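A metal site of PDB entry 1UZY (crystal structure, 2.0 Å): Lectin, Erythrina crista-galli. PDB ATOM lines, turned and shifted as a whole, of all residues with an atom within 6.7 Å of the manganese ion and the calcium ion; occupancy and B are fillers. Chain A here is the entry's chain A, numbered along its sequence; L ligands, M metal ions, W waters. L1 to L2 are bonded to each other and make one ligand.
O3 of LG2 L2 lies within hydrogen-bond range of OD1 of Asp 89.
The side-chain amide nitrogen (ND2) of Asn 133 sits at hydrogen-bond distance from an oxygen (O2) of LG2 L2 (2.9 Å).
The backbone NH (N) of Gly 107 lies within hydrogen-bond range of an oxygen (O2) of LG2 L2 (3.1 Å).
The side-chain carboxylate (OE1) of Glu 127 sits close to the side-chain carboxylate (OD2) of Asp 146, at 2.6 Å.
N of Glu 127 sits at hydrogen-bond distance from O of Gly 144 (2.8 Å).
Along chain A the residues within 4 Å of the manganese ion span positions 127 to 142.
The nearest printed residue that does not touch the manganese ion is Ser 152 (4.2 Å).
The manganese ion is bound by the side-chain carboxylate (OD2) of Asp 129 (2.1 Å), the side-chain carboxylate (OE2) of Glu 127 (2.2 Å), the side-chain carboxylate (OD1) of Asp 136 (2.2 Å), water W2 (2.2 Å), water W1 (2.3 Å) and a ring nitrogen (NE2) of His 142 (2.4 Å).
The calcium ion is bound by OD1 of Asn 133 (2.5 Å), OD2 of Asp 136 (2.5 Å), O of Phe 131 (2.5 Å), OD2 of Asp 129 (2.5 Å), water W3 (2.5 Å), water W4 (2.6 Å) and OD1 of Asp 129 (2.6 Å).
Water W1 bridges OE1 of Glu 127 and O of Ile 150.
Water W3 lies within hydrogen-bond range of the backbone carbonyl oxygen of Gly 107 and the indole nitrogen of Trp 135.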
ATOM      1  N   ASP A  89      -2.730   1.574  29.682  1.00  0.00           N
ATOM      2  CA  ASP A  89      -2.168   2.925  29.638  1.00  0.00           C
ATOM      3  C   ASP A  89      -2.253   3.513  28.228  1.00  0.00           C
ATOM      4  O   ASP A  89      -2.212   4.732  28.058  1.00  0.00           O
ATOM      5  CB  ASP A  89      -0.699   2.927  30.056  1.00  0.00           C
ATOM      6  CG  ASP A  89      -0.510   3.155  31.546  1.00  0.00           C
ATOM      7  OD1 ASP A  89      -0.328   2.159  32.270  1.00  0.00           O
ATOM      8  OD2 ASP A  89      -0.554   4.334  31.973  1.00  0.00           O
ATOM      9  N   TYR A 106       3.812   0.820  31.456  1.00  0.00           N
ATOM     10  CA  TYR A 106       2.843   1.737  32.043  1.00  0.00           C
ATOM     11  C   TYR A 106       2.729   2.999  31.182  1.00  0.00           C
ATOM     12  O   TYR A 106       2.603   2.898  29.964  1.00  0.00           O
ATOM     13  CB  TYR A 106       3.251   2.081  33.484  1.00  0.00           C
ATOM     14  CG  TYR A 106       3.473   0.853  34.349  1.00  0.00           C
ATOM     15  CD1 TYR A 106       4.372   0.883  35.425  1.00  0.00           C
ATOM     16  CD2 TYR A 106       2.818  -0.359  34.074  1.00  0.00           C
ATOM     17  CE1 TYR A 106       4.610  -0.255  36.202  1.00  0.00           C
ATOM     18  CE2 TYR A 106       3.056  -1.496  34.850  1.00  0.00           C
ATOM     19  CZ  TYR A 106       3.959  -1.436  35.904  1.00  0.00           C
ATOM     20  OH  TYR A 106       4.224  -2.561  36.667  1.00  0.00           O
ATOM     21  N   GLY A 107       2.784   4.163  31.813  1.00  0.00           N
ATOM     22  CA  GLY A 107       2.668   5.427  31.103  1.00  0.00           C
ATOM     23  C   GLY A 107       3.744   5.725  30.070  1.00  0.00           C
ATOM     24  O   GLY A 107       3.570   6.627  29.252  1.00  0.00           O
ATOM     25  N   TYR A 108       4.856   4.999  30.116  1.00  0.00           N
ATOM     26  CA  TYR A 108       5.930   5.227  29.143  1.00  0.00           C
ATOM     27  C   TYR A 108       5.646   4.445  27.857  1.00  0.00           C
ATOM     28  O   TYR A 108       6.397   4.521  26.880  1.00  0.00           O
ATOM     29  CB  TYR A 108       7.287   4.877  29.763  1.00  0.00           C
ATOM     30  CG  TYR A 108       7.563   5.719  30.987  1.00  0.00           C
ATOM     31  CD1 TYR A 108       7.479   7.110  30.928  1.00  0.00           C
ATOM     32  CD2 TYR A 108       7.844   5.138  32.223  1.00  0.00           C
ATOM     33  CE1 TYR A 108       7.648   7.900  32.058  1.00  0.00           C
ATOM     34  CE2 TYR A 108       8.020   5.929  33.375  1.00  0.00           C
ATOM     35  CZ  TYR A 108       7.924   7.314  33.282  1.00  0.00           C
ATOM     36  OH  TYR A 108       8.055   8.109  34.392  1.00  0.00           O
ATOM     37  N   LEU A 109       4.547   3.697  27.887  1.00  0.00           N
ATOM     38  CA  LEU A 109       4.054   2.928  26.732  1.00  0.00           C
ATOM     39  C   LEU A 109       5.035   2.005  26.024  1.00  0.00           C
ATOM     40  O   LEU A 109       4.855   1.696  24.850  1.00  0.00           O
ATOM     41  CB  LEU A 109       3.454   3.903  25.706  1.00  0.00           C
ATOM     42  CG  LEU A 109       2.436   4.918  26.263  1.00  0.00           C
ATOM     43  CD1 LEU A 109       1.954   5.843  25.152  1.00  0.00           C
ATOM     44  CD2 LEU A 109       1.264   4.173  26.861  1.00  0.00           C
ATOM     45  N   GLU A 127       0.998   8.975  20.101  1.00  0.00           N
ATOM     46  CA  GLU A 127       0.344   8.174  21.117  1.00  0.00           C
ATOM     47  C   GLU A 127      -1.172   8.297  21.177  1.00  0.00           C
ATOM     48  O   GLU A 127      -1.757   9.318  20.791  1.00  0.00           O
ATOM     49  CB  GLU A 127       0.902   8.549  22.501  1.00  0.00           C
ATOM     50  CG  GLU A 127       0.663  10.023  22.854  1.00  0.00           C
ATOM     51  CD  GLU A 127       0.995  10.336  24.293  1.00  0.00           C
ATOM     52  OE1 GLU A 127       2.140  10.074  24.712  1.00  0.00           O
ATOM     53  OE2 GLU A 127       0.110  10.855  25.009  1.00  0.00           O
ATOM     54  N   ASP A 129      -3.182   7.714  24.174  1.00  0.00           N
ATOM     55  CA  ASP A 129      -3.071   7.623  25.618  1.00  0.00           C
ATOM     56  C   ASP A 129      -4.382   7.524  26.406  1.00  0.00           C
ATOM     57  O   ASP A 129      -5.210   8.429  26.342  1.00  0.00           O
ATOM     58  CB  ASP A 129      -2.280   8.857  26.045  1.00  0.00           C
ATOM     59  CG  ASP A 129      -1.719   8.731  27.419  1.00  0.00           C
ATOM     60  OD1 ASP A 129      -2.227   7.880  28.180  1.00  0.00           O
ATOM     61  OD2 ASP A 129      -0.779   9.492  27.735  1.00  0.00           O
ATOM     62  N   THR A 130      -4.543   6.455  27.182  1.00  0.00           N
ATOM     63  CA  THR A 130      -5.770   6.207  27.953  1.00  0.00           C
ATOM     64  C   THR A 130      -5.774   6.506  29.458  1.00  0.00           C
ATOM     65  O   THR A 130      -6.829   6.450  30.093  1.00  0.00           O
ATOM     66  CB  THR A 130      -6.221   4.745  27.770  1.00  0.00           C
ATOM     67  OG1 THR A 130      -5.150   3.868  28.115  1.00  0.00           O
ATOM     68  CG2 THR A 130      -6.632   4.486  26.313  1.00  0.00           C
ATOM     69  N   PHE A 131      -4.613   6.801  30.034  1.00  0.00           N
ATOM     70  CA  PHE A 131      -4.535   7.104  31.469  1.00  0.00           C
ATOM     71  C   PHE A 131      -3.817   8.424  31.672  1.00  0.00           C
ATOM     72  O   PHE A 131      -2.768   8.652  31.098  1.00  0.00           O
ATOM     73  CB  PHE A 131      -3.751   6.011  32.207  1.00  0.00           C
ATOM     74  CG  PHE A 131      -3.628   6.244  33.686  1.00  0.00           C
ATOM     75  CD1 PHE A 131      -4.625   5.813  34.561  1.00  0.00           C
ATOM     76  CD2 PHE A 131      -2.540   6.940  34.200  1.00  0.00           C
ATOM     77  CE1 PHE A 131      -4.528   6.065  35.931  1.00  0.00           C
ATOM     78  CE2 PHE A 131      -2.442   7.201  35.573  1.00  0.00           C
ATOM     79  CZ  PHE A 131      -3.433   6.765  36.432  1.00  0.00           C
ATOM     80  N   SER A 132      -4.350   9.297  32.525  1.00  0.00           N
ATOM     81  CA  SER A 132      -3.693  10.577  32.740  1.00  0.00           C
ATOM     82  C   SER A 132      -2.606  10.542  33.816  1.00  0.00           C
ATOM     83  O   SER A 132      -2.904  10.496  35.009  1.00  0.00           O
ATOM     84  CB  SER A 132      -4.740  11.643  33.112  1.00  0.00           C
ATOM     85  OG  SER A 132      -4.138  12.908  33.257  1.00  0.00           O
ATOM     86  N   ASN A 133      -1.345  10.563  33.388  1.00  0.00           N
ATOM     87  CA  ASN A 133      -0.212  10.561  34.315  1.00  0.00           C
ATOM     88  C   ASN A 133       0.077  12.016  34.708  1.00  0.00           C
ATOM     89  O   ASN A 133      -0.503  12.953  34.154  1.00  0.00           O
ATOM     90  CB  ASN A 133       1.041   9.950  33.668  1.00  0.00           C
ATOM     91  CG  ASN A 133       0.871   8.475  33.353  1.00  0.00           C
ATOM     92  OD1 ASN A 133       0.452   8.120  32.257  1.00  0.00           O
ATOM     93  ND2 ASN A 133       1.205   7.612  34.299  1.00  0.00           N
ATOM     94  N   TRP A 135       2.404  13.979  33.987  1.00  0.00           N
ATOM     95  CA  TRP A 135       2.908  14.782  32.871  1.00  0.00           C
ATOM     96  C   TRP A 135       1.868  14.954  31.764  1.00  0.00           C
ATOM     97  O   TRP A 135       2.152  15.604  30.761  1.00  0.00           O
ATOM     98  CB  TRP A 135       4.148  14.116  32.282  1.00  0.00           C
ATOM     99  CG  TRP A 135       3.878  12.698  31.820  1.00  0.00           C
ATOM    100  CD1 TRP A 135       3.269  12.312  30.665  1.00  0.00           C
ATOM    101  CD2 TRP A 135       4.190  11.494  32.541  1.00  0.00           C
ATOM    102  NE1 TRP A 135       3.172  10.941  30.619  1.00  0.00           N
ATOM    103  CE2 TRP A 135       3.736  10.410  31.753  1.00  0.00           C
ATOM    104  CE3 TRP A 135       4.814  11.222  33.768  1.00  0.00           C
ATOM    105  CZ2 TRP A 135       3.873   9.087  32.151  1.00  0.00           C
ATOM    106  CZ3 TRP A 135       4.953   9.894  34.174  1.00  0.00           C
ATOM    107  CH2 TRP A 135       4.492   8.844  33.360  1.00  0.00           C
ATOM    108  N   ASP A 136       0.687  14.366  31.943  1.00  0.00           N
ATOM    109  CA  ASP A 136      -0.385  14.422  30.941  1.00  0.00           C
ATOM    110  C   ASP A 136      -1.460  15.464  31.171  1.00  0.00           C
ATOM    111  O   ASP A 136      -1.623  15.980  32.278  1.00  0.00           O
ATOM    112  CB  ASP A 136      -1.173  13.098  30.908  1.00  0.00           C
ATOM    113  CG  ASP A 136      -0.455  11.995  30.186  1.00  0.00           C
ATOM    114  OD1 ASP A 136       0.135  12.244  29.124  1.00  0.00           O
ATOM    115  OD2 ASP A 136      -0.514  10.872  30.708  1.00  0.00           O
ATOM    116  N   PRO A 137      -2.217  15.777  30.111  1.00  0.00           N
ATOM    117  CA  PRO A 137      -3.299  16.744  30.261  1.00  0.00           C
ATOM    118  C   PRO A 137      -4.307  15.893  31.044  1.00  0.00           C
ATOM    119  O   PRO A 137      -4.191  14.661  31.053  1.00  0.00           O
ATOM    120  CB  PRO A 137      -3.732  17.009  28.820  1.00  0.00           C
ATOM    121  CG  PRO A 137      -3.386  15.737  28.102  1.00  0.00           C
ATOM    122  CD  PRO A 137      -2.017  15.443  28.688  1.00  0.00           C
ATOM    123  N   VAL A 140      -8.573  12.164  29.053  1.00  0.00           N
ATOM    124  CA  VAL A 140      -8.196  10.888  28.462  1.00  0.00           C
ATOM    125  C   VAL A 140      -9.456  10.203  27.939  1.00  0.00           C
ATOM    126  O   VAL A 140     -10.531  10.311  28.532  1.00  0.00           O
ATOM    127  CB  VAL A 140      -7.505   9.925  29.476  1.00  0.00           C
ATOM    128  CG1 VAL A 140      -6.071  10.358  29.719  1.00  0.00           C
ATOM    129  CG2 VAL A 140      -8.283   9.903  30.777  1.00  0.00           C
ATOM    130  N   HIS A 142      -6.457  10.656  24.852  1.00  0.00           N
ATOM    131  CA  HIS A 142      -5.997  11.773  24.049  1.00  0.00           C
ATOM    132  C   HIS A 142      -4.914  11.309  23.100  1.00  0.00           C
ATOM    133  O   HIS A 142      -4.157  10.362  23.397  1.00  0.00           O
ATOM    134  CB  HIS A 142      -5.460  12.928  24.924  1.00  0.00           C
ATOM    135  CG  HIS A 142      -4.293  12.560  25.793  1.00  0.00           C
ATOM    136  ND1 HIS A 142      -4.422  12.289  27.135  1.00  0.00           N
ATOM    137  CD2 HIS A 142      -2.968  12.443  25.508  1.00  0.00           C
ATOM    138  CE1 HIS A 142      -3.233  12.022  27.653  1.00  0.00           C
ATOM    139  NE2 HIS A 142      -2.333  12.105  26.677  1.00  0.00           N
ATOM    140  N   ILE A 143      -4.868  11.941  21.922  1.00  0.00           N
ATOM    141  CA  ILE A 143      -3.844  11.642  20.943  1.00  0.00           C
ATOM    142  C   ILE A 143      -2.706  12.569  21.332  1.00  0.00           C
ATOM    143  O   ILE A 143      -2.946  13.670  21.841  1.00  0.00           O
ATOM    144  CB  ILE A 143      -4.270  12.024  19.508  1.00  0.00           C
ATOM    145  CG1 ILE A 143      -5.643  11.442  19.176  1.00  0.00           C
ATOM    146  CG2 ILE A 143      -3.214  11.526  18.517  1.00  0.00           C
ATOM    147  CD1 ILE A 143      -6.167  11.850  17.796  1.00  0.00           C
ATOM    148  N   GLY A 144      -1.474  12.135  21.110  1.00  0.00           N
ATOM    149  CA  GLY A 144      -0.342  12.971  21.457  1.00  0.00           C
ATOM    150  C   GLY A 144       0.818  12.818  20.493  1.00  0.00           C
ATOM    151  O   GLY A 144       1.082  11.722  19.989  1.00  0.00           O
ATOM    152  N   ASP A 146       4.645  12.954  20.345  1.00  0.00           N
ATOM    153  CA  ASP A 146       5.797  12.896  21.240  1.00  0.00           C
ATOM    154  C   ASP A 146       7.125  12.992  20.502  1.00  0.00           C
ATOM    155  O   ASP A 146       7.394  12.227  19.578  1.00  0.00           O
ATOM    156  CB  ASP A 146       5.784  11.592  22.041  1.00  0.00           C
ATOM    157  CG  ASP A 146       4.476  11.357  22.786  1.00  0.00           C
ATOM    158  OD1 ASP A 146       3.707  12.326  22.988  1.00  0.00           O
ATOM    159  OD2 ASP A 146       4.222  10.196  23.167  1.00  0.00           O
ATOM    160  N   ILE A 150       7.893  11.621  26.638  1.00  0.00           N
ATOM    161  CA  ILE A 150       6.534  11.142  26.811  1.00  0.00           C
ATOM    162  C   ILE A 150       5.647  12.366  27.079  1.00  0.00           C
ATOM    163  O   ILE A 150       4.419  12.281  27.075  1.00  0.00           O
ATOM    164  CB  ILE A 150       6.426  10.157  27.990  1.00  0.00           C
ATOM    165  CG1 ILE A 150       5.057   9.487  27.994  1.00  0.00           C
ATOM    166  CG2 ILE A 150       6.698  10.882  29.310  1.00  0.00           C
ATOM    167  CD1 ILE A 150       4.806   8.578  26.788  1.00  0.00           C
ATOM    168  N   ARG A 151       6.292  13.501  27.333  1.00  0.00           N
ATOM    169  CA  ARG A 151       5.591  14.756  27.557  1.00  0.00           C
ATOM    170  C   ARG A 151       5.312  15.335  26.169  1.00  0.00           C
ATOM    171  O   ARG A 151       6.135  16.051  25.601  1.00  0.00           O
ATOM    172  CB  ARG A 151       6.464  15.711  28.379  1.00  0.00           C
ATOM    173  CG  ARG A 151       6.757  15.237  29.800  1.00  0.00           C
ATOM    174  CD  ARG A 151       7.660  16.215  30.554  1.00  0.00           C
ATOM    175  NE  ARG A 151       8.040  15.685  31.863  1.00  0.00           N
ATOM    176  CZ  ARG A 151       7.334  15.825  32.987  1.00  0.00           C
ATOM    177  NH1 ARG A 151       6.180  16.486  32.980  1.00  0.00           N
ATOM    178  NH2 ARG A 151       7.767  15.277  34.109  1.00  0.00           N
ATOM    179  N   SER A 152       4.143  15.024  25.635  1.00  0.00           N
ATOM    180  CA  SER A 152       3.731  15.459  24.302  1.00  0.00           C
ATOM    181  C   SER A 152       3.899  16.949  24.013  1.00  0.00           C
ATOM    182  O   SER A 152       3.605  17.796  24.857  1.00  0.00           O
ATOM    183  CB  SER A 152       2.251  15.094  24.072  1.00  0.00           C
ATOM    184  OG  SER A 152       2.013  13.727  24.361  1.00  0.00           O
ATOM    185  N   THR A 155      -1.322  17.696  22.215  1.00  0.00           N
ATOM    186  CA  THR A 155      -2.290  16.640  22.506  1.00  0.00           C
ATOM    187  C   THR A 155      -3.681  17.033  22.032  1.00  0.00           C
ATOM    188  O   THR A 155      -3.994  18.217  21.878  1.00  0.00           O
ATOM    189  CB  THR A 155      -2.371  16.309  24.024  1.00  0.00           C
ATOM    190  OG1 THR A 155      -2.759  17.475  24.750  1.00  0.00           O
ATOM    191  CG2 THR A 155      -1.020  15.793  24.544  1.00  0.00           C
HETATM  192  C1  LIG L   1      -0.294   2.573  42.203  1.00  0.00           C
HETATM  193  C2  LIG L   1       0.143   2.386  40.751  1.00  0.00           C
HETATM  194  C3  LIG L   1       0.618   3.738  40.194  1.00  0.00           C
HETATM  195  C4  LIG L   1       1.803   4.252  41.075  1.00  0.00           C
HETATM  196  C5  LIG L   1       2.302   5.613  40.618  1.00  0.00           C
HETATM  197  C6  LIG L   1       0.912   3.088  43.020  1.00  0.00           C
HETATM  198  O1  LIG L   1       0.536   3.277  44.338  1.00  0.00           O
HETATM  199  O2  LIG L   1      -0.722   1.322  42.736  1.00  0.00           O
HETATM  200  O3  LIG L   1      -0.961   1.920  39.984  1.00  0.00           O
HETATM  201  O4  LIG L   1       1.050   3.587  38.819  1.00  0.00           O
HETATM  202  O5  LIG L   1       1.380   4.369  42.478  1.00  0.00           O
HETATM  203  O6  LIG L   1       3.440   6.015  41.367  1.00  0.00           O
HETATM  204  C1  LG2 L   2       0.195   4.042  37.799  1.00  0.00           C
HETATM  205  C2  LG2 L   2       1.003   4.129  36.486  1.00  0.00           C
HETATM  206  C3  LG2 L   2       0.086   4.625  35.344  1.00  0.00           C
HETATM  207  C4  LG2 L   2      -1.100   3.640  35.162  1.00  0.00           C
HETATM  208  C5  LG2 L   2      -1.832   3.577  36.543  1.00  0.00           C
HETATM  209  C6  LG2 L   2      -3.023   2.680  36.624  1.00  0.00           C
HETATM  210  O1  LG2 L   2       2.083   5.031  36.673  1.00  0.00           O
HETATM  211  O2  LG2 L   2       0.826   4.710  34.143  1.00  0.00           O
HETATM  212  O3  LG2 L   2      -0.603   2.355  34.805  1.00  0.00           O
HETATM  213  O4  LG2 L   2      -0.913   3.153  37.592  1.00  0.00           O
HETATM  214  O5  LG2 L   2      -3.552   2.732  37.938  1.00  0.00           O
HETATM  215 MN    MN M   1      -0.104  11.429  27.093  1.00  0.00          MN
HETATM  216 CA    CA M   2      -0.539   8.507  30.049  1.00  0.00          CA
HETATM  217  O   HOH W   1       2.137  10.819  27.190  1.00  0.00           O
HETATM  218  O   HOH W   2       0.549  13.473  26.567  1.00  0.00           O
HETATM  219  O   HOH W   3       1.791   8.550  29.033  1.00  0.00           O
HETATM  220  O   HOH W   4      -0.738   5.963  29.960  1.00  0.00           O
